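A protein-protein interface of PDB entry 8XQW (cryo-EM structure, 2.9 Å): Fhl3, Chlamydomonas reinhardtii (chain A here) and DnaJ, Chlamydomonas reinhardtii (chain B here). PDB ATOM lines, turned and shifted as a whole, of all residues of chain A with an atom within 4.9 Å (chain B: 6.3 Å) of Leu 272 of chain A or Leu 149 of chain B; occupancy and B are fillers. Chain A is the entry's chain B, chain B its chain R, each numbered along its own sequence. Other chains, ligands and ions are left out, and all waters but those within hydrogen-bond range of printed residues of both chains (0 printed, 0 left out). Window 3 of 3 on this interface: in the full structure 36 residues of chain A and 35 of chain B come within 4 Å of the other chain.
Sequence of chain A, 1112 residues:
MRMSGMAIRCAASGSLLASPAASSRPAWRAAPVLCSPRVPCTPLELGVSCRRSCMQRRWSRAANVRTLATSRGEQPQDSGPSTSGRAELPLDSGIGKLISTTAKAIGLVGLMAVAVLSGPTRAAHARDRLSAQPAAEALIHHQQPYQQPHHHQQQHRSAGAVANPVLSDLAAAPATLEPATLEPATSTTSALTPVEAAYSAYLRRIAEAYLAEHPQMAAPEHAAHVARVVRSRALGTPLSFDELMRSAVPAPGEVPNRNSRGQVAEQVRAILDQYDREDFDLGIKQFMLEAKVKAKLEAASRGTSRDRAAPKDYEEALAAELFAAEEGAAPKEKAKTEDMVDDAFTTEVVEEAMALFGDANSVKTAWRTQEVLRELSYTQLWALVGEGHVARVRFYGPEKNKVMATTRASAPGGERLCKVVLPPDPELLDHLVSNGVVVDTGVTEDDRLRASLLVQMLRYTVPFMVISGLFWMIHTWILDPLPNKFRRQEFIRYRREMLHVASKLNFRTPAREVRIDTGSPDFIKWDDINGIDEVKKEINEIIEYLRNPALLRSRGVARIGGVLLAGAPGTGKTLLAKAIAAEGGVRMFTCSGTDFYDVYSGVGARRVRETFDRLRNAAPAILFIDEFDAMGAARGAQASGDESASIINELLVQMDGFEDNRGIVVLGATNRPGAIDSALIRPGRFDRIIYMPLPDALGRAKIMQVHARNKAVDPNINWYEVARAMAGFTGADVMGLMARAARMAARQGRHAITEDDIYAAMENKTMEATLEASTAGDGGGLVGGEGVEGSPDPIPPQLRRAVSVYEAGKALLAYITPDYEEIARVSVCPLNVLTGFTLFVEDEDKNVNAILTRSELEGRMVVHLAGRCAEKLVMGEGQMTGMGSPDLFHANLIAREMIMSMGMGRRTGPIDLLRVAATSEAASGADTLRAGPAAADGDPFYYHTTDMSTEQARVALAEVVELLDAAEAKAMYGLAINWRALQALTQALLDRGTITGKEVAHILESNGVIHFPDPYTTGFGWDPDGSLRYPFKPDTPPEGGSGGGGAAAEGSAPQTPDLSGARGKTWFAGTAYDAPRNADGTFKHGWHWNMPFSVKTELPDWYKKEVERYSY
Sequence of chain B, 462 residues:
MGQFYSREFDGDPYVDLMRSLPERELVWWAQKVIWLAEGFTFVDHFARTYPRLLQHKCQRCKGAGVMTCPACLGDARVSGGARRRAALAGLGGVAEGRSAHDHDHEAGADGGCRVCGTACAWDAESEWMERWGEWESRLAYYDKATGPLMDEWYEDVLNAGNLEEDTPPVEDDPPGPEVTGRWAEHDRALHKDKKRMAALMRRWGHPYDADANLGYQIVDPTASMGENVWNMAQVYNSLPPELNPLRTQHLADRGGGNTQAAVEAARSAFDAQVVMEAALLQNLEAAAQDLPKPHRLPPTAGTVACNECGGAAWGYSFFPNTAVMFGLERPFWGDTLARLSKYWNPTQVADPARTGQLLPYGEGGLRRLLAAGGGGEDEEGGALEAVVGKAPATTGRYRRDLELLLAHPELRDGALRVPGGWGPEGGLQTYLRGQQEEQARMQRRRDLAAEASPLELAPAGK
Among the printed residues, pairs that only touch across the chains: Val 268 of chain A with Ala 145 of chain B, Leu 272 of chain A with Pro 148 of chain B, Leu 272 of chain A with Leu 149 of chain B, Leu 272 of chain A with Glu 152 of chain B and Glu 352 of chain A with Leu 149 of chain B.
Of chain B, only Pro 148 (3.4 Å), Leu 149 (3.7 Å) and Glu 152 (3.7 Å) come within 4 Å of Leu 272 of chain A.
Printed residues of chain A within 4 Å of Leu 149 of chain B: Leu 272 (3.7 Å) and Glu 352 (3.2 Å).
Of the printed residues of chain A, Ala 145 of chain B touches Val 268 (3.2 Å).
Of the printed residues of chain B, Glu 352 of chain A touches Leu 149.
Printed residues of chain B within 4 Å of Val 268 of chain A: Ala 145 (3.2 Å).
Of the printed residues of chain A, Pro 148 of chain B touches Leu 272 (3.4 Å).
Of the printed residues of chain A, Glu 152 of chain B touches Leu 272.
Tyr 275 of chain A touches none of the printed residues of chain B.
Trp 153 of chain B touches none of the printed residues of chain A.
The nearest printed residue of chain B that does not touch Leu 272 of chain A is Gly 147 of chain B (6.6 Å).
The nearest printed residue of chain B that does not touch Val 268 of chain A is Pro 148 of chain B (4.1 Å).
Printed residues of chain B that touch a printed residue of chain A: Ala 145, Pro 148, Leu 149 and Glu 152.
Hydrophobic or aromatic side chains of chain B within 4 Å of the printed part of chain A: Pro 148 and Leu 149.
Among the printed residues, 5 pairs touch across the chains.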
ATOM      1  N   VAL A 268      21.690  29.163 -16.543  1.00  0.00           N
ATOM      2  CA  VAL A 268      22.876  28.878 -15.738  1.00  0.00           C
ATOM      3  C   VAL A 268      24.109  29.499 -16.374  1.00  0.00           C
ATOM      4  O   VAL A 268      25.010  29.972 -15.673  1.00  0.00           O
ATOM      5  CB  VAL A 268      23.059  27.369 -15.502  1.00  0.00           C
ATOM      6  CG1 VAL A 268      21.773  26.747 -15.016  1.00  0.00           C
ATOM      7  CG2 VAL A 268      23.572  26.675 -16.738  1.00  0.00           C
ATOM      8  N   ARG A 269      24.162  29.545 -17.705  1.00  0.00           N
ATOM      9  CA  ARG A 269      25.314  30.180 -18.335  1.00  0.00           C
ATOM     10  C   ARG A 269      25.347  31.671 -18.034  1.00  0.00           C
ATOM     11  O   ARG A 269      26.404  32.220 -17.703  1.00  0.00           O
ATOM     12  CB  ARG A 269      25.305  29.934 -19.840  1.00  0.00           C
ATOM     13  CG  ARG A 269      26.137  28.746 -20.246  1.00  0.00           C
ATOM     14  CD  ARG A 269      25.944  28.385 -21.699  1.00  0.00           C
ATOM     15  NE  ARG A 269      26.916  27.383 -22.116  1.00  0.00           N
ATOM     16  CZ  ARG A 269      28.108  27.672 -22.625  1.00  0.00           C
ATOM     17  NH1 ARG A 269      28.471  28.936 -22.785  1.00  0.00           N
ATOM     18  NH2 ARG A 269      28.936  26.699 -22.974  1.00  0.00           N
ATOM     19  N   ALA A 270      24.197  32.340 -18.136  1.00  0.00           N
ATOM     20  CA  ALA A 270      24.155  33.773 -17.881  1.00  0.00           C
ATOM     21  C   ALA A 270      24.370  34.091 -16.411  1.00  0.00           C
ATOM     22  O   ALA A 270      24.720  35.223 -16.068  1.00  0.00           O
ATOM     23  CB  ALA A 270      22.826  34.351 -18.356  1.00  0.00           C
ATOM     24  N   ILE A 271      24.142  33.124 -15.528  1.00  0.00           N
ATOM     25  CA  ILE A 271      24.439  33.350 -14.119  1.00  0.00           C
ATOM     26  C   ILE A 271      25.916  33.140 -13.825  1.00  0.00           C
ATOM     27  O   ILE A 271      26.496  33.861 -13.005  1.00  0.00           O
ATOM     28  CB  ILE A 271      23.560  32.451 -13.238  1.00  0.00           C
ATOM     29  CG1 ILE A 271      22.305  33.197 -12.828  1.00  0.00           C
ATOM     30  CG2 ILE A 271      24.304  31.980 -12.007  1.00  0.00           C
ATOM     31  CD1 ILE A 271      21.508  32.454 -11.814  1.00  0.00           C
ATOM     32  N   LEU A 272      26.558  32.171 -14.477  1.00  0.00           N
ATOM     33  CA  LEU A 272      27.960  31.924 -14.170  1.00  0.00           C
ATOM     34  C   LEU A 272      28.878  32.940 -14.834  1.00  0.00           C
ATOM     35  O   LEU A 272      29.849  33.386 -14.217  1.00  0.00           O
ATOM     36  CB  LEU A 272      28.357  30.509 -14.572  1.00  0.00           C
ATOM     37  CG  LEU A 272      28.478  29.609 -13.345  1.00  0.00           C
ATOM     38  CD1 LEU A 272      27.130  29.442 -12.673  1.00  0.00           C
ATOM     39  CD2 LEU A 272      29.077  28.270 -13.702  1.00  0.00           C
ATOM     40  N   ASP A 273      28.589  33.351 -16.067  1.00  0.00           N
ATOM     41  CA  ASP A 273      29.476  34.323 -16.699  1.00  0.00           C
ATOM     42  C   ASP A 273      29.098  35.735 -16.272  1.00  0.00           C
ATOM     43  O   ASP A 273      29.438  36.713 -16.943  1.00  0.00           O
ATOM     44  CB  ASP A 273      29.472  34.179 -18.230  1.00  0.00           C
ATOM     45  CG  ASP A 273      28.175  34.645 -18.889  1.00  0.00           C
ATOM     46  OD1 ASP A 273      27.866  35.855 -18.871  1.00  0.00           O
ATOM     47  OD2 ASP A 273      27.472  33.795 -19.470  1.00  0.00           O
ATOM     48  N   GLN A 274      28.422  35.847 -15.134  1.00  0.00           N
ATOM     49  CA  GLN A 274      27.957  37.133 -14.645  1.00  0.00           C
ATOM     50  C   GLN A 274      29.091  38.083 -14.303  1.00  0.00           C
ATOM     51  O   GLN A 274      28.910  39.301 -14.388  1.00  0.00           O
ATOM     52  CB  GLN A 274      27.078  36.919 -13.416  1.00  0.00           C
ATOM     53  CG  GLN A 274      26.224  38.091 -13.025  1.00  0.00           C
ATOM     54  CD  GLN A 274      25.415  37.784 -11.793  1.00  0.00           C
ATOM     55  OE1 GLN A 274      24.674  38.626 -11.293  1.00  0.00           O
ATOM     56  NE2 GLN A 274      25.548  36.563 -11.295  1.00  0.00           N
ATOM     57  N   TYR A 275      30.254  37.557 -13.934  1.00  0.00           N
ATOM     58  CA  TYR A 275      31.356  38.380 -13.453  1.00  0.00           C
ATOM     59  C   TYR A 275      32.621  38.181 -14.278  1.00  0.00           C
ATOM     60  O   TYR A 275      33.445  39.089 -14.393  1.00  0.00           O
ATOM     61  CB  TYR A 275      31.636  38.067 -11.986  1.00  0.00           C
ATOM     62  CG  TYR A 275      30.471  38.368 -11.077  1.00  0.00           C
ATOM     63  CD1 TYR A 275      29.807  39.579 -11.152  1.00  0.00           C
ATOM     64  CD2 TYR A 275      30.034  37.440 -10.149  1.00  0.00           C
ATOM     65  CE1 TYR A 275      28.746  39.860 -10.327  1.00  0.00           C
ATOM     66  CE2 TYR A 275      28.974  37.711  -9.321  1.00  0.00           C
ATOM     67  CZ  TYR A 275      28.332  38.923  -9.413  1.00  0.00           C
ATOM     68  OH  TYR A 275      27.269  39.201  -8.585  1.00  0.00           O
ATOM     69  N   GLU A 352      21.308  30.629  -8.094  1.00  0.00           N
ATOM     70  CA  GLU A 352      21.599  29.315  -8.642  1.00  0.00           C
ATOM     71  C   GLU A 352      20.760  28.242  -7.963  1.00  0.00           C
ATOM     72  O   GLU A 352      20.335  27.280  -8.613  1.00  0.00           O
ATOM     73  CB  GLU A 352      23.086  29.010  -8.514  1.00  0.00           C
ATOM     74  CG  GLU A 352      23.605  28.146  -9.637  1.00  0.00           C
ATOM     75  CD  GLU A 352      22.998  26.760  -9.645  1.00  0.00           C
ATOM     76  OE1 GLU A 352      22.771  26.199  -8.553  1.00  0.00           O
ATOM     77  OE2 GLU A 352      22.715  26.241 -10.746  1.00  0.00           O
ATOM     78  N   LEU A 356      17.713  25.590 -10.313  1.00  0.00           N
ATOM     79  CA  LEU A 356      17.971  24.135 -10.262  1.00  0.00           C
ATOM     80  C   LEU A 356      16.771  23.443  -9.613  1.00  0.00           C
ATOM     81  O   LEU A 356      16.307  22.430 -10.163  1.00  0.00           O
ATOM     82  CB  LEU A 356      19.242  23.896  -9.461  1.00  0.00           C
ATOM     83  CG  LEU A 356      20.352  23.113 -10.165  1.00  0.00           C
ATOM     84  CD1 LEU A 356      21.610  23.120  -9.317  1.00  0.00           C
ATOM     85  CD2 LEU A 356      19.903  21.688 -10.426  1.00  0.00           C
ATOM     86  N   ALA B 145      22.637  20.887 -19.683  1.00  0.00           N
ATOM     87  CA  ALA B 145      22.194  22.162 -19.133  1.00  0.00           C
ATOM     88  C   ALA B 145      23.047  22.574 -17.947  1.00  0.00           C
ATOM     89  O   ALA B 145      23.494  23.722 -17.867  1.00  0.00           O
ATOM     90  CB  ALA B 145      20.727  22.082 -18.726  1.00  0.00           C
ATOM     91  N   THR B 146      23.291  21.650 -17.018  1.00  0.00           N
ATOM     92  CA  THR B 146      24.081  21.910 -15.822  1.00  0.00           C
ATOM     93  C   THR B 146      25.577  21.797 -16.073  1.00  0.00           C
ATOM     94  O   THR B 146      26.353  21.685 -15.118  1.00  0.00           O
ATOM     95  CB  THR B 146      23.663  20.956 -14.710  1.00  0.00           C
ATOM     96  OG1 THR B 146      23.527  19.637 -15.250  1.00  0.00           O
ATOM     97  CG2 THR B 146      22.337  21.395 -14.125  1.00  0.00           C
ATOM     98  N   GLY B 147      25.999  21.827 -17.343  1.00  0.00           N
ATOM     99  CA  GLY B 147      27.384  21.681 -17.723  1.00  0.00           C
ATOM    100  C   GLY B 147      28.383  22.558 -16.977  1.00  0.00           C
ATOM    101  O   GLY B 147      29.399  22.039 -16.518  1.00  0.00           O
ATOM    102  N   PRO B 148      28.137  23.863 -16.858  1.00  0.00           N
ATOM    103  CA  PRO B 148      29.143  24.713 -16.188  1.00  0.00           C
ATOM    104  C   PRO B 148      29.399  24.357 -14.730  1.00  0.00           C
ATOM    105  O   PRO B 148      30.554  24.409 -14.281  1.00  0.00           O
ATOM    106  CB  PRO B 148      28.546  26.117 -16.335  1.00  0.00           C
ATOM    107  CG  PRO B 148      27.690  26.035 -17.529  1.00  0.00           C
ATOM    108  CD  PRO B 148      27.102  24.668 -17.519  1.00  0.00           C
ATOM    109  N   LEU B 149      28.364  23.999 -13.971  1.00  0.00           N
ATOM    110  CA  LEU B 149      28.581  23.616 -12.578  1.00  0.00           C
ATOM    111  C   LEU B 149      29.392  22.333 -12.479  1.00  0.00           C
ATOM    112  O   LEU B 149      30.347  22.254 -11.695  1.00  0.00           O
ATOM    113  CB  LEU B 149      27.249  23.452 -11.854  1.00  0.00           C
ATOM    114  CG  LEU B 149      26.302  24.646 -11.766  1.00  0.00           C
ATOM    115  CD1 LEU B 149      25.385  24.458 -10.587  1.00  0.00           C
ATOM    116  CD2 LEU B 149      27.065  25.937 -11.637  1.00  0.00           C
ATOM    117  N   MET B 150      29.019  21.314 -13.253  1.00  0.00           N
ATOM    118  CA  MET B 150      29.809  20.091 -13.277  1.00  0.00           C
ATOM    119  C   MET B 150      31.239  20.375 -13.706  1.00  0.00           C
ATOM    120  O   MET B 150      32.176  19.748 -13.210  1.00  0.00           O
ATOM    121  CB  MET B 150      29.170  19.064 -14.208  1.00  0.00           C
ATOM    122  CG  MET B 150      27.726  18.735 -13.893  1.00  0.00           C
ATOM    123  SD  MET B 150      27.496  17.871 -12.334  1.00  0.00           S
ATOM    124  CE  MET B 150      25.850  17.209 -12.569  1.00  0.00           C
ATOM    125  N   ASP B 151      31.431  21.334 -14.611  1.00  0.00           N
ATOM    126  CA  ASP B 151      32.776  21.632 -15.091  1.00  0.00           C
ATOM    127  C   ASP B 151      33.622  22.264 -13.996  1.00  0.00           C
ATOM    128  O   ASP B 151      34.775  21.866 -13.782  1.00  0.00           O
ATOM    129  CB  ASP B 151      32.708  22.545 -16.309  1.00  0.00           C
ATOM    130  CG  ASP B 151      32.696  21.771 -17.607  1.00  0.00           C
ATOM    131  OD1 ASP B 151      32.721  20.523 -17.546  1.00  0.00           O
ATOM    132  OD2 ASP B 151      32.664  22.402 -18.685  1.00  0.00           O
ATOM    133  N   GLU B 152      33.075  23.257 -13.299  1.00  0.00           N
ATOM    134  CA  GLU B 152      33.839  23.881 -12.227  1.00  0.00           C
ATOM    135  C   GLU B 152      34.117  22.894 -11.100  1.00  0.00           C
ATOM    136  O   GLU B 152      35.215  22.900 -10.533  1.00  0.00           O
ATOM    137  CB  GLU B 152      33.114  25.125 -11.710  1.00  0.00           C
ATOM    138  CG  GLU B 152      32.112  24.880 -10.599  1.00  0.00           C
ATOM    139  CD  GLU B 152      31.237  26.085 -10.327  1.00  0.00           C
ATOM    140  OE1 GLU B 152      31.389  27.104 -11.032  1.00  0.00           O
ATOM    141  OE2 GLU B 152      30.393  26.016  -9.411  1.00  0.00           O
ATOM    142  N   TRP B 153      33.169  22.008 -10.796  1.00  0.00           N
ATOM    143  CA  TRP B 153      33.406  21.020  -9.749  1.00  0.00           C
ATOM    144  C   TRP B 153      34.449  19.997 -10.181  1.00  0.00           C
ATOM    145  O   TRP B 153      35.282  19.574  -9.374  1.00  0.00           O
ATOM    146  CB  TRP B 153      32.092  20.345  -9.391  1.00  0.00           C
ATOM    147  CG  TRP B 153      32.197  19.190  -8.474  1.00  0.00           C
ATOM    148  CD1 TRP B 153      33.110  18.999  -7.487  1.00  0.00           C
ATOM    149  CD2 TRP B 153      31.322  18.061  -8.437  1.00  0.00           C
ATOM    150  NE1 TRP B 153      32.868  17.812  -6.845  1.00  0.00           N
ATOM    151  CE2 TRP B 153      31.772  17.218  -7.413  1.00  0.00           C
ATOM    152  CE3 TRP B 153      30.202  17.682  -9.181  1.00  0.00           C
ATOM    153  CZ2 TRP B 153      31.143  16.019  -7.111  1.00  0.00           C
ATOM    154  CZ3 TRP B 153      29.582  16.492  -8.880  1.00  0.00           C
ATOM    155  CH2 TRP B 153      30.051  15.674  -7.856  1.00  0.00           C
ATOM    156  N   TYR B 154      34.428  19.596 -11.450  1.00  0.00           N
ATOM    157  CA  TYR B 154      35.428  18.663 -11.957  1.00  0.00           C
ATOM    158  C   TYR B 154      36.815  19.282 -11.936  1.00  0.00           C
ATOM    159  O   TYR B 154      37.792  18.618 -11.577  1.00  0.00           O
ATOM    160  CB  TYR B 154      35.052  18.239 -13.372  1.00  0.00           C
ATOM    161  CG  TYR B 154      36.011  17.291 -14.036  1.00  0.00           C
ATOM    162  CD1 TYR B 154      35.957  15.934 -13.781  1.00  0.00           C
ATOM    163  CD2 TYR B 154      36.946  17.747 -14.946  1.00  0.00           C
ATOM    164  CE1 TYR B 154      36.820  15.060 -14.395  1.00  0.00           C
ATOM    165  CE2 TYR B 154      37.813  16.881 -15.567  1.00  0.00           C
ATOM    166  CZ  TYR B 154      37.746  15.537 -15.288  1.00  0.00           C
ATOM    167  OH  TYR B 154      38.608  14.662 -15.903  1.00  0.00           O
ATOM    168  N   HIS B 206      33.092  11.211  -9.971  1.00  0.00           N
ATOM    169  CA  HIS B 206      32.560  12.349 -10.693  1.00  0.00           C
ATOM    170  C   HIS B 206      31.902  11.837 -11.969  1.00  0.00           C
ATOM    171  O   HIS B 206      32.442  10.926 -12.610  1.00  0.00           O
ATOM    172  CB  HIS B 206      33.665  13.344 -11.024  1.00  0.00           C
ATOM    173  CG  HIS B 206      33.168  14.614 -11.635  1.00  0.00           C
ATOM    174  ND1 HIS B 206      32.910  14.739 -12.983  1.00  0.00           N
ATOM    175  CD2 HIS B 206      32.875  15.816 -11.083  1.00  0.00           C
ATOM    176  CE1 HIS B 206      32.486  15.963 -13.236  1.00  0.00           C
ATOM    177  NE2 HIS B 206      32.456  16.636 -12.101  1.00  0.00           N
